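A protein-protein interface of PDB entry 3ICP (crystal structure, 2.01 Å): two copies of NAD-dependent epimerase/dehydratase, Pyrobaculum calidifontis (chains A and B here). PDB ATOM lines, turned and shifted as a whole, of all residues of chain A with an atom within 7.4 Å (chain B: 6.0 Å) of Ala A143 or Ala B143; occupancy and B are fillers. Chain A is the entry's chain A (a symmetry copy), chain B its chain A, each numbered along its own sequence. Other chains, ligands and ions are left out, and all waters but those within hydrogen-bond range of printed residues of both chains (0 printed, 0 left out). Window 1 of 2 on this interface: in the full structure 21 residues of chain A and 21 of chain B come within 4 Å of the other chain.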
ATOM      1  N   PHE A  86       7.279 -12.795   3.997  1.00  0.00           N
ATOM      2  CA  PHE A  86       8.681 -13.194   4.100  1.00  0.00           C
ATOM      3  C   PHE A  86       9.100 -13.482   5.535  1.00  0.00           C
ATOM      4  O   PHE A  86       9.669 -14.534   5.821  1.00  0.00           O
ATOM      5  CB  PHE A  86       9.597 -12.098   3.541  1.00  0.00           C
ATOM      6  CG  PHE A  86      11.058 -12.444   3.599  1.00  0.00           C
ATOM      7  CD1 PHE A  86      11.613 -13.350   2.696  1.00  0.00           C
ATOM      8  CD2 PHE A  86      11.881 -11.885   4.573  1.00  0.00           C
ATOM      9  CE1 PHE A  86      12.964 -13.697   2.763  1.00  0.00           C
ATOM     10  CE2 PHE A  86      13.235 -12.226   4.651  1.00  0.00           C
ATOM     11  CZ  PHE A  86      13.774 -13.129   3.749  1.00  0.00           C
ATOM     12  N   ASN A  89       7.158 -16.478   7.233  1.00  0.00           N
ATOM     13  CA  ASN A  89       7.407 -17.781   6.632  1.00  0.00           C
ATOM     14  C   ASN A  89       8.887 -18.138   6.517  1.00  0.00           C
ATOM     15  O   ASN A  89       9.358 -19.082   7.157  1.00  0.00           O
ATOM     16  CB  ASN A  89       6.752 -17.860   5.250  1.00  0.00           C
ATOM     17  CG  ASN A  89       5.233 -17.871   5.326  1.00  0.00           C
ATOM     18  OD1 ASN A  89       4.583 -16.830   5.214  1.00  0.00           O
ATOM     19  ND2 ASN A  89       4.661 -19.052   5.532  1.00  0.00           N
ATOM     20  N   VAL A  90       9.622 -17.386   5.710  1.00  0.00           N
ATOM     21  CA  VAL A  90      11.038 -17.666   5.514  1.00  0.00           C
ATOM     22  C   VAL A  90      11.895 -17.471   6.754  1.00  0.00           C
ATOM     23  O   VAL A  90      12.674 -18.354   7.125  1.00  0.00           O
ATOM     24  CB  VAL A  90      11.650 -16.795   4.398  1.00  0.00           C
ATOM     25  CG1 VAL A  90      13.068 -17.250   4.153  1.00  0.00           C
ATOM     26  CG2 VAL A  90      10.834 -16.904   3.120  1.00  0.00           C
ATOM     27  N   THR A  93      10.784 -19.893   9.650  1.00  0.00           N
ATOM     28  CA  THR A  93      11.204 -21.259   9.359  1.00  0.00           C
ATOM     29  C   THR A  93      12.698 -21.445   9.562  1.00  0.00           C
ATOM     30  O   THR A  93      13.133 -22.467  10.091  1.00  0.00           O
ATOM     31  CB  THR A  93      10.805 -21.663   7.921  1.00  0.00           C
ATOM     32  OG1 THR A  93       9.377 -21.637   7.811  1.00  0.00           O
ATOM     33  CG2 THR A  93      11.302 -23.072   7.585  1.00  0.00           C
ATOM     34  N   LEU A  97      14.557 -24.029  12.129  1.00  0.00           N
ATOM     35  CA  LEU A  97      15.598 -24.974  11.717  1.00  0.00           C
ATOM     36  C   LEU A  97      16.871 -24.836  12.564  1.00  0.00           C
ATOM     37  O   LEU A  97      17.483 -25.836  12.944  1.00  0.00           O
ATOM     38  CB  LEU A  97      15.924 -24.769  10.232  1.00  0.00           C
ATOM     39  CG  LEU A  97      14.816 -25.188   9.261  1.00  0.00           C
ATOM     40  CD1 LEU A  97      15.106 -24.672   7.850  1.00  0.00           C
ATOM     41  CD2 LEU A  97      14.706 -26.707   9.277  1.00  0.00           C
ATOM     42  N   PHE A 110       7.294 -30.124   8.371  1.00  0.00           N
ATOM     43  CA  PHE A 110       6.972 -28.782   7.880  1.00  0.00           C
ATOM     44  C   PHE A 110       5.655 -28.688   7.127  1.00  0.00           C
ATOM     45  O   PHE A 110       5.415 -29.434   6.180  1.00  0.00           O
ATOM     46  CB  PHE A 110       8.105 -28.288   6.966  1.00  0.00           C
ATOM     47  CG  PHE A 110       7.881 -26.905   6.399  1.00  0.00           C
ATOM     48  CD1 PHE A 110       7.587 -25.830   7.235  1.00  0.00           C
ATOM     49  CD2 PHE A 110       8.004 -26.667   5.029  1.00  0.00           C
ATOM     50  CE1 PHE A 110       7.421 -24.542   6.722  1.00  0.00           C
ATOM     51  CE2 PHE A 110       7.841 -25.388   4.502  1.00  0.00           C
ATOM     52  CZ  PHE A 110       7.547 -24.319   5.354  1.00  0.00           C
ATOM     53  N   VAL A 116       3.305 -23.758  -3.622  1.00  0.00           N
ATOM     54  CA  VAL A 116       4.685 -23.851  -4.079  1.00  0.00           C
ATOM     55  C   VAL A 116       4.705 -24.200  -5.572  1.00  0.00           C
ATOM     56  O   VAL A 116       5.699 -23.966  -6.263  1.00  0.00           O
ATOM     57  CB  VAL A 116       5.482 -24.923  -3.296  1.00  0.00           C
ATOM     58  CG1 VAL A 116       5.460 -24.583  -1.807  1.00  0.00           C
ATOM     59  CG2 VAL A 116       4.911 -26.326  -3.553  1.00  0.00           C
ATOM     60  N   TYR A 131       8.957 -25.920  -8.571  1.00  0.00           N
ATOM     61  CA  TYR A 131       8.466 -24.735  -7.880  1.00  0.00           C
ATOM     62  C   TYR A 131       8.186 -23.642  -8.903  1.00  0.00           C
ATOM     63  O   TYR A 131       9.076 -23.254  -9.667  1.00  0.00           O
ATOM     64  CB  TYR A 131       9.520 -24.199  -6.908  1.00  0.00           C
ATOM     65  CG  TYR A 131       9.899 -25.119  -5.777  1.00  0.00           C
ATOM     66  CD1 TYR A 131       8.933 -25.648  -4.921  1.00  0.00           C
ATOM     67  CD2 TYR A 131      11.239 -25.415  -5.521  1.00  0.00           C
ATOM     68  CE1 TYR A 131       9.295 -26.444  -3.836  1.00  0.00           C
ATOM     69  CE2 TYR A 131      11.608 -26.209  -4.440  1.00  0.00           C
ATOM     70  CZ  TYR A 131      10.633 -26.718  -3.603  1.00  0.00           C
ATOM     71  OH  TYR A 131      11.012 -27.505  -2.536  1.00  0.00           O
ATOM     72  N   PRO A 133       5.846 -20.772  -7.895  1.00  0.00           N
ATOM     73  CA  PRO A 133       4.915 -19.936  -7.137  1.00  0.00           C
ATOM     74  C   PRO A 133       4.659 -18.584  -7.794  1.00  0.00           C
ATOM     75  O   PRO A 133       5.561 -17.994  -8.396  1.00  0.00           O
ATOM     76  CB  PRO A 133       5.596 -19.808  -5.774  1.00  0.00           C
ATOM     77  CG  PRO A 133       7.056 -19.831  -6.128  1.00  0.00           C
ATOM     78  CD  PRO A 133       7.133 -20.917  -7.186  1.00  0.00           C
ATOM     79  N   TYR A 137       3.838 -15.556  -0.752  1.00  0.00           N
ATOM     80  CA  TYR A 137       3.601 -16.620   0.221  1.00  0.00           C
ATOM     81  C   TYR A 137       4.117 -17.954  -0.336  1.00  0.00           C
ATOM     82  O   TYR A 137       4.829 -18.693   0.352  1.00  0.00           O
ATOM     83  CB  TYR A 137       2.106 -16.729   0.505  1.00  0.00           C
ATOM     84  CG  TYR A 137       1.759 -17.512   1.745  1.00  0.00           C
ATOM     85  CD1 TYR A 137       1.502 -16.860   2.951  1.00  0.00           C
ATOM     86  CD2 TYR A 137       1.639 -18.901   1.709  1.00  0.00           C
ATOM     87  CE1 TYR A 137       1.122 -17.574   4.091  1.00  0.00           C
ATOM     88  CE2 TYR A 137       1.262 -19.628   2.851  1.00  0.00           C
ATOM     89  CZ  TYR A 137       0.998 -18.953   4.033  1.00  0.00           C
ATOM     90  OH  TYR A 137       0.573 -19.650   5.145  1.00  0.00           O
ATOM     91  N   GLY A 138       3.740 -18.254  -1.577  1.00  0.00           N
ATOM     92  CA  GLY A 138       4.179 -19.487  -2.216  1.00  0.00           C
ATOM     93  C   GLY A 138       5.689 -19.549  -2.364  1.00  0.00           C
ATOM     94  O   GLY A 138       6.282 -20.617  -2.235  1.00  0.00           O
ATOM     95  N   ALA A 139       6.324 -18.417  -2.650  1.00  0.00           N
ATOM     96  CA  ALA A 139       7.778 -18.406  -2.782  1.00  0.00           C
ATOM     97  C   ALA A 139       8.384 -18.644  -1.398  1.00  0.00           C
ATOM     98  O   ALA A 139       9.404 -19.324  -1.262  1.00  0.00           O
ATOM     99  CB  ALA A 139       8.264 -17.064  -3.339  1.00  0.00           C
ATOM    100  N   ALA A 140       7.749 -18.090  -0.371  1.00  0.00           N
ATOM    101  CA  ALA A 140       8.251 -18.246   0.986  1.00  0.00           C
ATOM    102  C   ALA A 140       8.178 -19.702   1.432  1.00  0.00           C
ATOM    103  O   ALA A 140       9.115 -20.205   2.054  1.00  0.00           O
ATOM    104  CB  ALA A 140       7.478 -17.340   1.947  1.00  0.00           C
ATOM    105  N   LYS A 141       7.077 -20.386   1.116  1.00  0.00           N
ATOM    106  CA  LYS A 141       6.943 -21.792   1.476  1.00  0.00           C
ATOM    107  C   LYS A 141       7.971 -22.624   0.707  1.00  0.00           C
ATOM    108  O   LYS A 141       8.584 -23.539   1.268  1.00  0.00           O
ATOM    109  CB  LYS A 141       5.529 -22.288   1.168  1.00  0.00           C
ATOM    110  CG  LYS A 141       4.467 -21.806   2.161  1.00  0.00           C
ATOM    111  CD  LYS A 141       4.750 -22.373   3.557  1.00  0.00           C
ATOM    112  CE  LYS A 141       3.606 -22.110   4.540  1.00  0.00           C
ATOM    113  NZ  LYS A 141       3.876 -22.712   5.890  1.00  0.00           N
ATOM    114  N   ALA A 142       8.172 -22.310  -0.568  1.00  0.00           N
ATOM    115  CA  ALA A 142       9.147 -23.037  -1.379  1.00  0.00           C
ATOM    116  C   ALA A 142      10.543 -22.841  -0.777  1.00  0.00           C
ATOM    117  O   ALA A 142      11.311 -23.797  -0.643  1.00  0.00           O
ATOM    118  CB  ALA A 142       9.106 -22.542  -2.827  1.00  0.00           C
ATOM    119  N   ALA A 143      10.866 -21.607  -0.403  1.00  0.00           N
ATOM    120  CA  ALA A 143      12.161 -21.310   0.208  1.00  0.00           C
ATOM    121  C   ALA A 143      12.287 -22.075   1.527  1.00  0.00           C
ATOM    122  O   ALA A 143      13.361 -22.562   1.877  1.00  0.00           O
ATOM    123  CB  ALA A 143      12.294 -19.818   0.455  1.00  0.00           C
ATOM    124  N   GLY A 144      11.187 -22.169   2.264  1.00  0.00           N
ATOM    125  CA  GLY A 144      11.217 -22.899   3.518  1.00  0.00           C
ATOM    126  C   GLY A 144      11.570 -24.352   3.242  1.00  0.00           C
ATOM    127  O   GLY A 144      12.367 -24.957   3.961  1.00  0.00           O
ATOM    128  N   GLU A 145      10.972 -24.915   2.197  1.00  0.00           N
ATOM    129  CA  GLU A 145      11.239 -26.300   1.816  1.00  0.00           C
ATOM    130  C   GLU A 145      12.716 -26.514   1.475  1.00  0.00           C
ATOM    131  O   GLU A 145      13.335 -27.479   1.934  1.00  0.00           O
ATOM    132  CB  GLU A 145      10.372 -26.710   0.618  1.00  0.00           C
ATOM    133  CG  GLU A 145       8.929 -27.095   0.969  1.00  0.00           C
ATOM    134  CD  GLU A 145       8.254 -27.828  -0.173  1.00  0.00           C
ATOM    135  OE1 GLU A 145       8.986 -28.351  -1.040  1.00  0.00           O
ATOM    136  OE2 GLU A 145       7.006 -27.906  -0.198  1.00  0.00           O
ATOM    137  N   VAL A 146      13.284 -25.627   0.666  1.00  0.00           N
ATOM    138  CA  VAL A 146      14.692 -25.743   0.276  1.00  0.00           C
ATOM    139  C   VAL A 146      15.598 -25.751   1.496  1.00  0.00           C
ATOM    140  O   VAL A 146      16.515 -26.565   1.584  1.00  0.00           O
ATOM    141  CB  VAL A 146      15.102 -24.591  -0.665  1.00  0.00           C
ATOM    142  CG1 VAL A 146      16.620 -24.625  -0.955  1.00  0.00           C
ATOM    143  CG2 VAL A 146      14.316 -24.710  -1.953  1.00  0.00           C
ATOM    144  N   MET A 147      15.332 -24.848   2.441  1.00  0.00           N
ATOM    145  CA  MET A 147      16.130 -24.772   3.659  1.00  0.00           C
ATOM    146  C   MET A 147      15.980 -26.041   4.501  1.00  0.00           C
ATOM    147  O   MET A 147      16.969 -26.554   5.030  1.00  0.00           O
ATOM    148  CB  MET A 147      15.730 -23.549   4.488  1.00  0.00           C
ATOM    149  CG  MET A 147      16.029 -22.228   3.805  1.00  0.00           C
ATOM    150  SD  MET A 147      15.860 -20.820   4.911  1.00  0.00           S
ATOM    151  CE  MET A 147      14.042 -20.752   5.080  1.00  0.00           C
ATOM    152  N   CYS A 148      14.749 -26.539   4.630  1.00  0.00           N
ATOM    153  CA  CYS A 148      14.486 -27.763   5.399  1.00  0.00           C
ATOM    154  C   CYS A 148      15.228 -28.960   4.823  1.00  0.00           C
ATOM    155  O   CYS A 148      15.794 -29.765   5.562  1.00  0.00           O
ATOM    156  CB  CYS A 148      12.994 -28.117   5.399  1.00  0.00           C
ATOM    157  SG  CYS A 148      11.947 -27.116   6.474  1.00  0.00           S
ATOM    158  N   ALA A 149      15.185 -29.091   3.501  1.00  0.00           N
ATOM    159  CA  ALA A 149      15.835 -30.205   2.818  1.00  0.00           C
ATOM    160  C   ALA A 149      17.340 -30.134   3.013  1.00  0.00           C
ATOM    161  O   ALA A 149      18.003 -31.153   3.186  1.00  0.00           O
ATOM    162  CB  ALA A 149      15.491 -30.187   1.323  1.00  0.00           C
ATOM    163  N   VAL B  90      19.645 -14.563   1.831  1.00  0.00           N
ATOM    164  CA  VAL B  90      18.192 -14.569   1.724  1.00  0.00           C
ATOM    165  C   VAL B  90      17.529 -13.250   2.088  1.00  0.00           C
ATOM    166  O   VAL B  90      16.703 -12.731   1.331  1.00  0.00           O
ATOM    167  CB  VAL B  90      17.551 -15.658   2.609  1.00  0.00           C
ATOM    168  CG1 VAL B  90      16.070 -15.700   2.327  1.00  0.00           C
ATOM    169  CG2 VAL B  90      18.180 -17.014   2.334  1.00  0.00           C
ATOM    170  N   GLY B 138      24.403 -22.431  -0.142  1.00  0.00           N
ATOM    171  CA  GLY B 138      23.742 -22.931  -1.339  1.00  0.00           C
ATOM    172  C   GLY B 138      22.229 -22.893  -1.216  1.00  0.00           C
ATOM    173  O   GLY B 138      21.533 -22.624  -2.191  1.00  0.00           O
ATOM    174  N   ALA B 139      21.703 -23.173  -0.027  1.00  0.00           N
ATOM    175  CA  ALA B 139      20.256 -23.130   0.162  1.00  0.00           C
ATOM    176  C   ALA B 139      19.807 -21.671   0.072  1.00  0.00           C
ATOM    177  O   ALA B 139      18.739 -21.369  -0.465  1.00  0.00           O
ATOM    178  CB  ALA B 139      19.868 -23.711   1.525  1.00  0.00           C
ATOM    179  N   ALA B 140      20.630 -20.766   0.591  1.00  0.00           N
ATOM    180  CA  ALA B 140      20.290 -19.351   0.568  1.00  0.00           C
ATOM    181  C   ALA B 140      20.243 -18.823  -0.861  1.00  0.00           C
ATOM    182  O   ALA B 140      19.339 -18.061  -1.209  1.00  0.00           O
ATOM    183  CB  ALA B 140      21.282 -18.551   1.416  1.00  0.00           C
ATOM    184  N   LYS B 141      21.204 -19.223  -1.694  1.00  0.00           N
ATOM    185  CA  LYS B 141      21.214 -18.791  -3.086  1.00  0.00           C
ATOM    186  C   LYS B 141      20.003 -19.375  -3.818  1.00  0.00           C
ATOM    187  O   LYS B 141      19.362 -18.686  -4.618  1.00  0.00           O
ATOM    188  CB  LYS B 141      22.507 -19.234  -3.773  1.00  0.00           C
ATOM    189  CG  LYS B 141      23.737 -18.409  -3.381  1.00  0.00           C
ATOM    190  CD  LYS B 141      23.568 -16.955  -3.837  1.00  0.00           C
ATOM    191  CE  LYS B 141      24.851 -16.136  -3.673  1.00  0.00           C
ATOM    192  NZ  LYS B 141      24.685 -14.727  -4.168  1.00  0.00           N
ATOM    193  N   ALA B 142      19.681 -20.634  -3.544  1.00  0.00           N
ATOM    194  CA  ALA B 142      18.530 -21.273  -4.181  1.00  0.00           C
ATOM    195  C   ALA B 142      17.256 -20.522  -3.779  1.00  0.00           C
ATOM    196  O   ALA B 142      16.402 -20.235  -4.622  1.00  0.00           O
ATOM    197  CB  ALA B 142      18.446 -22.745  -3.768  1.00  0.00           C
ATOM    198  N   ALA B 143      17.134 -20.193  -2.497  1.00  0.00           N
ATOM    199  CA  ALA B 143      15.972 -19.452  -2.007  1.00  0.00           C
ATOM    200  C   ALA B 143      15.925 -18.080  -2.683  1.00  0.00           C
ATOM    201  O   ALA B 143      14.854 -17.572  -3.012  1.00  0.00           O
ATOM    202  CB  ALA B 143      16.053 -19.288  -0.501  1.00  0.00           C
ATOM    203  N   GLY B 144      17.091 -17.476  -2.880  1.00  0.00           N
ATOM    204  CA  GLY B 144      17.133 -16.183  -3.537  1.00  0.00           C
ATOM    205  C   GLY B 144      16.575 -16.318  -4.945  1.00  0.00           C
ATOM    206  O   GLY B 144      15.810 -15.471  -5.407  1.00  0.00           O
ATOM    207  N   GLU B 145      16.963 -17.388  -5.631  1.00  0.00           N
ATOM    208  CA  GLU B 145      16.486 -17.643  -6.988  1.00  0.00           C
ATOM    209  C   GLU B 145      14.962 -17.790  -7.029  1.00  0.00           C
ATOM    210  O   GLU B 145      14.295 -17.198  -7.883  1.00  0.00           O
ATOM    211  CB  GLU B 145      17.137 -18.908  -7.564  1.00  0.00           C
ATOM    212  CG  GLU B 145      18.556 -18.708  -8.111  1.00  0.00           C
ATOM    213  CD  GLU B 145      18.987 -19.872  -8.981  1.00  0.00           C
ATOM    214  OE1 GLU B 145      18.094 -20.609  -9.449  1.00  0.00           O
ATOM    215  OE2 GLU B 145      20.204 -20.042  -9.218  1.00  0.00           O
ATOM    216  N   VAL B 146      14.407 -18.581  -6.118  1.00  0.00           N
ATOM    217  CA  VAL B 146      12.956 -18.790  -6.073  1.00  0.00           C
ATOM    218  C   VAL B 146      12.219 -17.473  -5.905  1.00  0.00           C
ATOM    219  O   VAL B 146      11.230 -17.222  -6.590  1.00  0.00           O
ATOM    220  CB  VAL B 146      12.571 -19.749  -4.927  1.00  0.00           C
ATOM    221  CG1 VAL B 146      11.037 -19.851  -4.781  1.00  0.00           C
ATOM    222  CG2 VAL B 146      13.167 -21.111  -5.209  1.00  0.00           C
ATOM    223  N   MET B 147      12.709 -16.628  -4.998  1.00  0.00           N
ATOM    224  CA  MET B 147      12.088 -15.330  -4.760  1.00  0.00           C
ATOM    225  C   MET B 147      12.191 -14.431  -5.993  1.00  0.00           C
ATOM    226  O   MET B 147      11.223 -13.755  -6.350  1.00  0.00           O
ATOM    227  CB  MET B 147      12.735 -14.637  -3.558  1.00  0.00           C
ATOM    228  CG  MET B 147      12.512 -15.363  -2.245  1.00  0.00           C
ATOM    229  SD  MET B 147      12.989 -14.381  -0.816  1.00  0.00           S
ATOM    230  CE  MET B 147      14.808 -14.436  -0.972  1.00  0.00           C
ATOM    231  N   CYS B 148      13.359 -14.419  -6.637  1.00  0.00           N
ATOM    232  CA  CYS B 148      13.569 -13.609  -7.845  1.00  0.00           C
ATOM    233  C   CYS B 148      12.621 -14.012  -8.965  1.00  0.00           C
ATOM    234  O   CYS B 148      12.062 -13.159  -9.654  1.00  0.00           O
ATOM    235  CB  CYS B 148      14.996 -13.764  -8.385  1.00  0.00           C
ATOM    236  SG  CYS B 148      16.283 -12.891  -7.473  1.00  0.00           S
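Along chain A the printed residues that touch a printed residue of chain B span positions 86 to 146.
Of the 12 printed residues of chain B, 6 touch a printed residue of chain A.
Hydrophobic or aromatic side chains of chain B within 4 Å of the printed part of chain A: Val B90, Ala B142, Ala B143, Val B146 and Met B147.
Among the printed residues, no Asp or Glu carboxylate lies within 4 Å of a Lys or Arg side-chain nitrogen of the other chain.
Val A90 touches its own counterpart, Val B90.
Ala A139 touches Val B146, and with the chains exchanged Val A146 touches Ala B139.
Ala A142 touches Val B146, and with the chains exchanged Val A146 touches Ala B142.
Ala B143 touches its own counterpart, Ala A143.
12 positions are printed for both chains.
Of the printed residues of chain B, Ala A143 touches Ala B143 (3.9 Å).
Ala B143 touches just one residue of chain A: Ala A143 (3.9 Å).
Of chain A, only Val A146 comes within 4 Å of Ala B142.
Gly B144 touches none of the printed residues of chain A.
Of the printed residues of chain B, Val A90 touches Val B90 (3.8 Å).
Of the printed residues of chain B, Phe A86 touches Val B90 and Met B147.
The nearest residue of chain A that does not touch Ala B143 is Val A146 (4.7 Å).
Among the printed residues, merely in contact across the chains: Phe A86 with Met B147 (3.6 Å), Phe A86 with Val B90 (3.7 Å), Val A90 with Val B90 (3.8 Å), Val A146 with Ala B142 (3.8 Å), Ala A142 with Val B146 (3.8 Å), Ala A143 with Ala B143 (3.9 Å), Ala A139 with Val B146 (3.9 Å) and Val A146 with Ala B139 (3.9 Å).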
